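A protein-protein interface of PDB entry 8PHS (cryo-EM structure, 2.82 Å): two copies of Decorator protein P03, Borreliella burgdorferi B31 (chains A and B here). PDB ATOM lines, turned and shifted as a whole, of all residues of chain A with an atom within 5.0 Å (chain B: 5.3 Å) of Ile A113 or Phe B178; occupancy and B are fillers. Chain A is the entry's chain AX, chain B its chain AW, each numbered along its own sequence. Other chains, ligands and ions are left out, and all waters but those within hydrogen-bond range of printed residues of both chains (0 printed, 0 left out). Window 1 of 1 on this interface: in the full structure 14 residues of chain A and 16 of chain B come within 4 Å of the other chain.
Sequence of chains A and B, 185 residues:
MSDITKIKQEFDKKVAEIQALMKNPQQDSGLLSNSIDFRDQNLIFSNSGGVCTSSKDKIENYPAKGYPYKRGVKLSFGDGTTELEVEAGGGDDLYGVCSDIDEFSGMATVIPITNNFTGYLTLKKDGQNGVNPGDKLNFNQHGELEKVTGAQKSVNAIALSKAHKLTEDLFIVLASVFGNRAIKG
The side-chain amide oxygen (OD1) of Asn B180 lies close to the side-chain amide oxygen (OD1) of Asn B156.
The backbone carbonyl oxygen of Asn B156 is in hydrogen-bond range of the backbone NH of Phe B178, at 3.3 Å.
N of Val B155 sits at hydrogen-bond distance from O of Arg B181, 3.2 Å away.
The backbone NH of Ile A113 sits at hydrogen-bond distance from the backbone carbonyl oxygen of Tyr A95, at 3.1 Å.
OH of Tyr A95 touches ND2 of Asn B116, 3.97 Å away.
Ile A113 touches Phe B178.
Asn B116 touches Thr A114.
O of Phe B178 touches CG2 of Thr A114, 3.3 Å away.
Hydrophobic or aromatic side chains of chain A that line the printed part of chain B: Tyr A95 and Ile A113.
Among the printed residues, 7 pairs touch across the chains.
Among the printed residues, no Asp or Glu carboxylate lies within 4 Å of a Lys or Arg side-chain nitrogen of the other chain.
Asn A180 touches its own counterpart, Asn B180.
Positions printed for both chains: 113, 155, 177, 179 and 180.
Of the 7 pairs that touch across the chains among the printed residues, 1 has its exchanged pair printed and touching as well.
O of Asn B180 is in hydrogen-bond range of ND2 of Asn A180 (3.1 Å).
NH2 of Arg B181 sits at hydrogen-bond distance from O of Leu A94 (2.7 Å).
The guanidinium group of Arg B181 is in hydrogen-bond range of the side-chain amide oxygen of Asn A180, 3.2 Å away.
Ile A113 touches just one residue of chain B: Phe B178.
Of chain A, only Ile A113 (3.7 Å) and Thr A114 (3.3 Å) come within 4 Å of Phe B178.
Printed residues of chain B within 4 Å of Leu A94: Arg B181 (2.7 Å).
Printed residues of chain B within 4 Å of Asn A180: Asn B180 and Arg B181.
Printed residues of chain B within 4 Å of Thr A114: Asn B116 (3.7 Å) and Phe B178 (3.3 Å).
Of the printed residues of chain A, Asn B180 touches Asn A180 (3.1 Å).
Printed residues of chain B within 4 Å of Tyr A95: Asn B116 (3.97 Å).
The nearest residue of chain A that does not touch Phe B178 is Tyr A95 (4.5 Å).
The nearest printed residue of chain B that does not touch Tyr A95 is Phe B178 (4.5 Å).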
ATOM      1  N   LEU A  94      11.160  -8.920 -19.533  1.00  0.00           N
ATOM      2  CA  LEU A  94      10.019  -9.783 -19.252  1.00  0.00           C
ATOM      3  C   LEU A  94       8.810  -8.964 -18.822  1.00  0.00           C
ATOM      4  O   LEU A  94       8.899  -8.130 -17.917  1.00  0.00           O
ATOM      5  CB  LEU A  94      10.385 -10.797 -18.170  1.00  0.00           C
ATOM      6  CG  LEU A  94       9.228 -11.648 -17.645  1.00  0.00           C
ATOM      7  CD1 LEU A  94       8.816 -12.691 -18.670  1.00  0.00           C
ATOM      8  CD2 LEU A  94       9.602 -12.305 -16.328  1.00  0.00           C
ATOM      9  N   TYR A  95       7.678  -9.210 -19.477  1.00  0.00           N
ATOM     10  CA  TYR A  95       6.416  -8.551 -19.171  1.00  0.00           C
ATOM     11  C   TYR A  95       5.426  -9.472 -18.475  1.00  0.00           C
ATOM     12  O   TYR A  95       4.766  -9.057 -17.518  1.00  0.00           O
ATOM     13  CB  TYR A  95       5.790  -8.005 -20.459  1.00  0.00           C
ATOM     14  CG  TYR A  95       4.481  -7.277 -20.264  1.00  0.00           C
ATOM     15  CD1 TYR A  95       4.424  -6.087 -19.553  1.00  0.00           C
ATOM     16  CD2 TYR A  95       3.302  -7.779 -20.796  1.00  0.00           C
ATOM     17  CE1 TYR A  95       3.229  -5.417 -19.377  1.00  0.00           C
ATOM     18  CE2 TYR A  95       2.103  -7.118 -20.624  1.00  0.00           C
ATOM     19  CZ  TYR A  95       2.072  -5.938 -19.913  1.00  0.00           C
ATOM     20  OH  TYR A  95       0.878  -5.277 -19.740  1.00  0.00           O
ATOM     21  N   GLY A  96       5.319 -10.713 -18.926  1.00  0.00           N
ATOM     22  CA  GLY A  96       4.398 -11.646 -18.322  1.00  0.00           C
ATOM     23  C   GLY A  96       4.588 -13.037 -18.877  1.00  0.00           C
ATOM     24  O   GLY A  96       5.599 -13.337 -19.514  1.00  0.00           O
ATOM     25  N   ILE A 111      -0.708 -13.221 -18.523  1.00  0.00           N
ATOM     26  CA  ILE A 111      -0.873 -12.884 -17.112  1.00  0.00           C
ATOM     27  C   ILE A 111       0.291 -11.981 -16.717  1.00  0.00           C
ATOM     28  O   ILE A 111       1.447 -12.421 -16.794  1.00  0.00           O
ATOM     29  CB  ILE A 111      -0.921 -14.140 -16.232  1.00  0.00           C
ATOM     30  CG1 ILE A 111      -2.175 -14.957 -16.545  1.00  0.00           C
ATOM     31  CG2 ILE A 111      -0.879 -13.762 -14.762  1.00  0.00           C
ATOM     32  CD1 ILE A 111      -2.414 -16.100 -15.589  1.00  0.00           C
ATOM     33  N   PRO A 112       0.043 -10.738 -16.311  1.00  0.00           N
ATOM     34  CA  PRO A 112       1.149  -9.821 -16.016  1.00  0.00           C
ATOM     35  C   PRO A 112       2.026 -10.335 -14.885  1.00  0.00           C
ATOM     36  O   PRO A 112       1.602 -11.123 -14.038  1.00  0.00           O
ATOM     37  CB  PRO A 112       0.437  -8.522 -15.617  1.00  0.00           C
ATOM     38  CG  PRO A 112      -0.908  -8.619 -16.247  1.00  0.00           C
ATOM     39  CD  PRO A 112      -1.266 -10.074 -16.215  1.00  0.00           C
ATOM     40  N   ILE A 113       3.280  -9.874 -14.888  1.00  0.00           N
ATOM     41  CA  ILE A 113       4.240 -10.298 -13.876  1.00  0.00           C
ATOM     42  C   ILE A 113       3.822  -9.855 -12.481  1.00  0.00           C
ATOM     43  O   ILE A 113       4.284 -10.427 -11.487  1.00  0.00           O
ATOM     44  CB  ILE A 113       5.644  -9.770 -14.227  1.00  0.00           C
ATOM     45  CG1 ILE A 113       6.720 -10.541 -13.461  1.00  0.00           C
ATOM     46  CG2 ILE A 113       5.746  -8.282 -13.941  1.00  0.00           C
ATOM     47  CD1 ILE A 113       6.772 -12.012 -13.797  1.00  0.00           C
ATOM     48  N   THR A 114       2.946  -8.856 -12.376  1.00  0.00           N
ATOM     49  CA  THR A 114       2.441  -8.407 -11.086  1.00  0.00           C
ATOM     50  C   THR A 114       1.411  -9.357 -10.491  1.00  0.00           C
ATOM     51  O   THR A 114       1.019  -9.173  -9.334  1.00  0.00           O
ATOM     52  CB  THR A 114       1.828  -7.011 -11.217  1.00  0.00           C
ATOM     53  OG1 THR A 114       0.916  -6.989 -12.322  1.00  0.00           O
ATOM     54  CG2 THR A 114       2.914  -5.975 -11.443  1.00  0.00           C
ATOM     55  N   ASN A 115       0.963 -10.353 -11.248  1.00  0.00           N
ATOM     56  CA  ASN A 115      -0.002 -11.341 -10.787  1.00  0.00           C
ATOM     57  C   ASN A 115       0.693 -12.694 -10.717  1.00  0.00           C
ATOM     58  O   ASN A 115       1.274 -13.145 -11.709  1.00  0.00           O
ATOM     59  CB  ASN A 115      -1.208 -11.394 -11.725  1.00  0.00           C
ATOM     60  CG  ASN A 115      -2.344 -12.225 -11.170  1.00  0.00           C
ATOM     61  OD1 ASN A 115      -2.250 -12.782 -10.078  1.00  0.00           O
ATOM     62  ND2 ASN A 115      -3.429 -12.313 -11.927  1.00  0.00           N
ATOM     63  N   VAL A 155      13.898 -12.662 -11.355  1.00  0.00           N
ATOM     64  CA  VAL A 155      12.490 -13.034 -11.325  1.00  0.00           C
ATOM     65  C   VAL A 155      12.319 -14.182 -10.343  1.00  0.00           C
ATOM     66  O   VAL A 155      13.083 -15.154 -10.378  1.00  0.00           O
ATOM     67  CB  VAL A 155      11.975 -13.435 -12.721  1.00  0.00           C
ATOM     68  CG1 VAL A 155      10.513 -13.840 -12.655  1.00  0.00           C
ATOM     69  CG2 VAL A 155      12.170 -12.294 -13.703  1.00  0.00           C
ATOM     70  N   VAL A 177       5.420 -18.584 -10.133  1.00  0.00           N
ATOM     71  CA  VAL A 177       6.063 -17.293 -10.351  1.00  0.00           C
ATOM     72  C   VAL A 177       5.355 -16.272  -9.476  1.00  0.00           C
ATOM     73  O   VAL A 177       4.127 -16.136  -9.545  1.00  0.00           O
ATOM     74  CB  VAL A 177       6.016 -16.877 -11.830  1.00  0.00           C
ATOM     75  CG1 VAL A 177       6.670 -15.519 -12.019  1.00  0.00           C
ATOM     76  CG2 VAL A 177       6.691 -17.926 -12.696  1.00  0.00           C
ATOM     77  N   GLY A 179       6.566 -12.774  -8.940  1.00  0.00           N
ATOM     78  CA  GLY A 179       7.064 -11.422  -9.110  1.00  0.00           C
ATOM     79  C   GLY A 179       8.562 -11.362  -9.334  1.00  0.00           C
ATOM     80  O   GLY A 179       9.256 -12.373  -9.477  1.00  0.00           O
ATOM     81  N   ASN A 180       9.057 -10.128  -9.373  1.00  0.00           N
ATOM     82  CA  ASN A 180      10.471  -9.868  -9.583  1.00  0.00           C
ATOM     83  C   ASN A 180      11.241  -9.974  -8.269  1.00  0.00           C
ATOM     84  O   ASN A 180      10.667 -10.107  -7.184  1.00  0.00           O
ATOM     85  CB  ASN A 180      10.675  -8.490 -10.209  1.00  0.00           C
ATOM     86  CG  ASN A 180       9.974  -8.346 -11.544  1.00  0.00           C
ATOM     87  OD1 ASN A 180      10.281  -9.058 -12.499  1.00  0.00           O
ATOM     88  ND2 ASN A 180       9.027  -7.420 -11.619  1.00  0.00           N
ATOM     89  N   ILE B 113       1.429   0.108  -6.763  1.00  0.00           N
ATOM     90  CA  ILE B 113       2.499  -0.360  -7.633  1.00  0.00           C
ATOM     91  C   ILE B 113       2.448  -1.869  -7.826  1.00  0.00           C
ATOM     92  O   ILE B 113       2.999  -2.386  -8.803  1.00  0.00           O
ATOM     93  CB  ILE B 113       3.868   0.086  -7.078  1.00  0.00           C
ATOM     94  CG1 ILE B 113       4.930   0.046  -8.177  1.00  0.00           C
ATOM     95  CG2 ILE B 113       4.279  -0.777  -5.896  1.00  0.00           C
ATOM     96  CD1 ILE B 113       4.556   0.834  -9.411  1.00  0.00           C
ATOM     97  N   ASN B 116      -0.538  -3.552 -12.153  1.00  0.00           N
ATOM     98  CA  ASN B 116      -0.062  -2.912 -13.370  1.00  0.00           C
ATOM     99  C   ASN B 116      -1.093  -1.918 -13.898  1.00  0.00           C
ATOM    100  O   ASN B 116      -2.305  -2.120 -13.786  1.00  0.00           O
ATOM    101  CB  ASN B 116       0.266  -3.958 -14.435  1.00  0.00           C
ATOM    102  CG  ASN B 116      -0.971  -4.563 -15.058  1.00  0.00           C
ATOM    103  OD1 ASN B 116      -1.825  -5.105 -14.361  1.00  0.00           O
ATOM    104  ND2 ASN B 116      -1.071  -4.478 -16.378  1.00  0.00           N
ATOM    105  N   VAL B 155      13.873   0.626 -13.445  1.00  0.00           N
ATOM    106  CA  VAL B 155      12.913   0.916 -14.504  1.00  0.00           C
ATOM    107  C   VAL B 155      11.522   0.557 -14.006  1.00  0.00           C
ATOM    108  O   VAL B 155      11.314  -0.534 -13.460  1.00  0.00           O
ATOM    109  CB  VAL B 155      13.252   0.153 -15.795  1.00  0.00           C
ATOM    110  CG1 VAL B 155      12.164   0.359 -16.834  1.00  0.00           C
ATOM    111  CG2 VAL B 155      14.598   0.611 -16.332  1.00  0.00           C
ATOM    112  N   ASN B 156      10.575   1.470 -14.187  1.00  0.00           N
ATOM    113  CA  ASN B 156       9.210   1.264 -13.721  1.00  0.00           C
ATOM    114  C   ASN B 156       8.185   1.175 -14.839  1.00  0.00           C
ATOM    115  O   ASN B 156       7.237   0.394 -14.728  1.00  0.00           O
ATOM    116  CB  ASN B 156       8.808   2.384 -12.752  1.00  0.00           C
ATOM    117  CG  ASN B 156       9.610   2.357 -11.470  1.00  0.00           C
ATOM    118  OD1 ASN B 156      10.351   1.408 -11.208  1.00  0.00           O
ATOM    119  ND2 ASN B 156       9.471   3.400 -10.662  1.00  0.00           N
ATOM    120  N   ALA B 157       8.336   1.941 -15.918  1.00  0.00           N
ATOM    121  CA  ALA B 157       7.334   1.960 -16.973  1.00  0.00           C
ATOM    122  C   ALA B 157       8.003   1.893 -18.339  1.00  0.00           C
ATOM    123  O   ALA B 157       9.211   2.095 -18.479  1.00  0.00           O
ATOM    124  CB  ALA B 157       6.448   3.209 -16.878  1.00  0.00           C
ATOM    125  N   ILE B 158       7.193   1.611 -19.356  1.00  0.00           N
ATOM    126  CA  ILE B 158       7.634   1.587 -20.743  1.00  0.00           C
ATOM    127  C   ILE B 158       6.692   2.463 -21.554  1.00  0.00           C
ATOM    128  O   ILE B 158       5.470   2.287 -21.493  1.00  0.00           O
ATOM    129  CB  ILE B 158       7.668   0.154 -21.306  1.00  0.00           C
ATOM    130  CG1 ILE B 158       8.794  -0.646 -20.650  1.00  0.00           C
ATOM    131  CG2 ILE B 158       7.832   0.173 -22.817  1.00  0.00           C
ATOM    132  CD1 ILE B 158       9.005  -2.016 -21.251  1.00  0.00           C
ATOM    133  N   SER B 176       2.964   2.047 -19.778  1.00  0.00           N
ATOM    134  CA  SER B 176       2.514   0.867 -19.050  1.00  0.00           C
ATOM    135  C   SER B 176       3.452   0.632 -17.876  1.00  0.00           C
ATOM    136  O   SER B 176       4.664   0.492 -18.065  1.00  0.00           O
ATOM    137  CB  SER B 176       2.476  -0.362 -19.957  1.00  0.00           C
ATOM    138  OG  SER B 176       1.526  -0.202 -20.991  1.00  0.00           O
ATOM    139  N   VAL B 177       2.890   0.585 -16.673  1.00  0.00           N
ATOM    140  CA  VAL B 177       3.651   0.332 -15.456  1.00  0.00           C
ATOM    141  C   VAL B 177       3.562  -1.153 -15.137  1.00  0.00           C
ATOM    142  O   VAL B 177       2.463  -1.715 -15.067  1.00  0.00           O
ATOM    143  CB  VAL B 177       3.128   1.181 -14.286  1.00  0.00           C
ATOM    144  CG1 VAL B 177       4.106   1.143 -13.125  1.00  0.00           C
ATOM    145  CG2 VAL B 177       2.884   2.612 -14.738  1.00  0.00           C
ATOM    146  N   PHE B 178       4.715  -1.791 -14.953  1.00  0.00           N
ATOM    147  CA  PHE B 178       4.778  -3.220 -14.686  1.00  0.00           C
ATOM    148  C   PHE B 178       5.316  -3.551 -13.301  1.00  0.00           C
ATOM    149  O   PHE B 178       5.494  -4.732 -12.988  1.00  0.00           O
ATOM    150  CB  PHE B 178       5.623  -3.921 -15.760  1.00  0.00           C
ATOM    151  CG  PHE B 178       7.013  -3.361 -15.911  1.00  0.00           C
ATOM    152  CD1 PHE B 178       8.008  -3.662 -14.993  1.00  0.00           C
ATOM    153  CD2 PHE B 178       7.323  -2.532 -16.976  1.00  0.00           C
ATOM    154  CE1 PHE B 178       9.281  -3.146 -15.134  1.00  0.00           C
ATOM    155  CE2 PHE B 178       8.595  -2.015 -17.122  1.00  0.00           C
ATOM    156  CZ  PHE B 178       9.575  -2.322 -16.201  1.00  0.00           C
ATOM    157  N   GLY B 179       5.586  -2.546 -12.464  1.00  0.00           N
ATOM    158  CA  GLY B 179       6.084  -2.763 -11.121  1.00  0.00           C
ATOM    159  C   GLY B 179       7.488  -2.203 -10.954  1.00  0.00           C
ATOM    160  O   GLY B 179       7.784  -1.088 -11.409  1.00  0.00           O
ATOM    161  N   ASN B 180       8.346  -2.976 -10.298  1.00  0.00           N
ATOM    162  CA  ASN B 180       9.731  -2.600 -10.057  1.00  0.00           C
ATOM    163  C   ASN B 180      10.660  -3.672 -10.608  1.00  0.00           C
ATOM    164  O   ASN B 180      10.419  -4.868 -10.426  1.00  0.00           O
ATOM    165  CB  ASN B 180      10.002  -2.397  -8.564  1.00  0.00           C
ATOM    166  CG  ASN B 180       9.575  -1.029  -8.076  1.00  0.00           C
ATOM    167  OD1 ASN B 180       9.087  -0.207  -8.850  1.00  0.00           O
ATOM    168  ND2 ASN B 180       9.761  -0.776  -6.786  1.00  0.00           N
ATOM    169  N   ARG B 181      11.721  -3.232 -11.281  1.00  0.00           N
ATOM    170  CA  ARG B 181      12.720  -4.139 -11.824  1.00  0.00           C
ATOM    171  C   ARG B 181      14.078  -3.457 -11.761  1.00  0.00           C
ATOM    172  O   ARG B 181      14.188  -2.256 -12.021  1.00  0.00           O
ATOM    173  CB  ARG B 181      12.387  -4.543 -13.264  1.00  0.00           C
ATOM    174  CG  ARG B 181      13.377  -5.516 -13.879  1.00  0.00           C
ATOM    175  CD  ARG B 181      12.869  -6.081 -15.194  1.00  0.00           C
ATOM    176  NE  ARG B 181      11.729  -6.971 -15.007  1.00  0.00           N
ATOM    177  CZ  ARG B 181      10.564  -6.836 -15.626  1.00  0.00           C
ATOM    178  NH1 ARG B 181      10.354  -5.864 -16.497  1.00  0.00           N
ATOM    179  NH2 ARG B 181       9.589  -7.703 -15.369  1.00  0.00           N
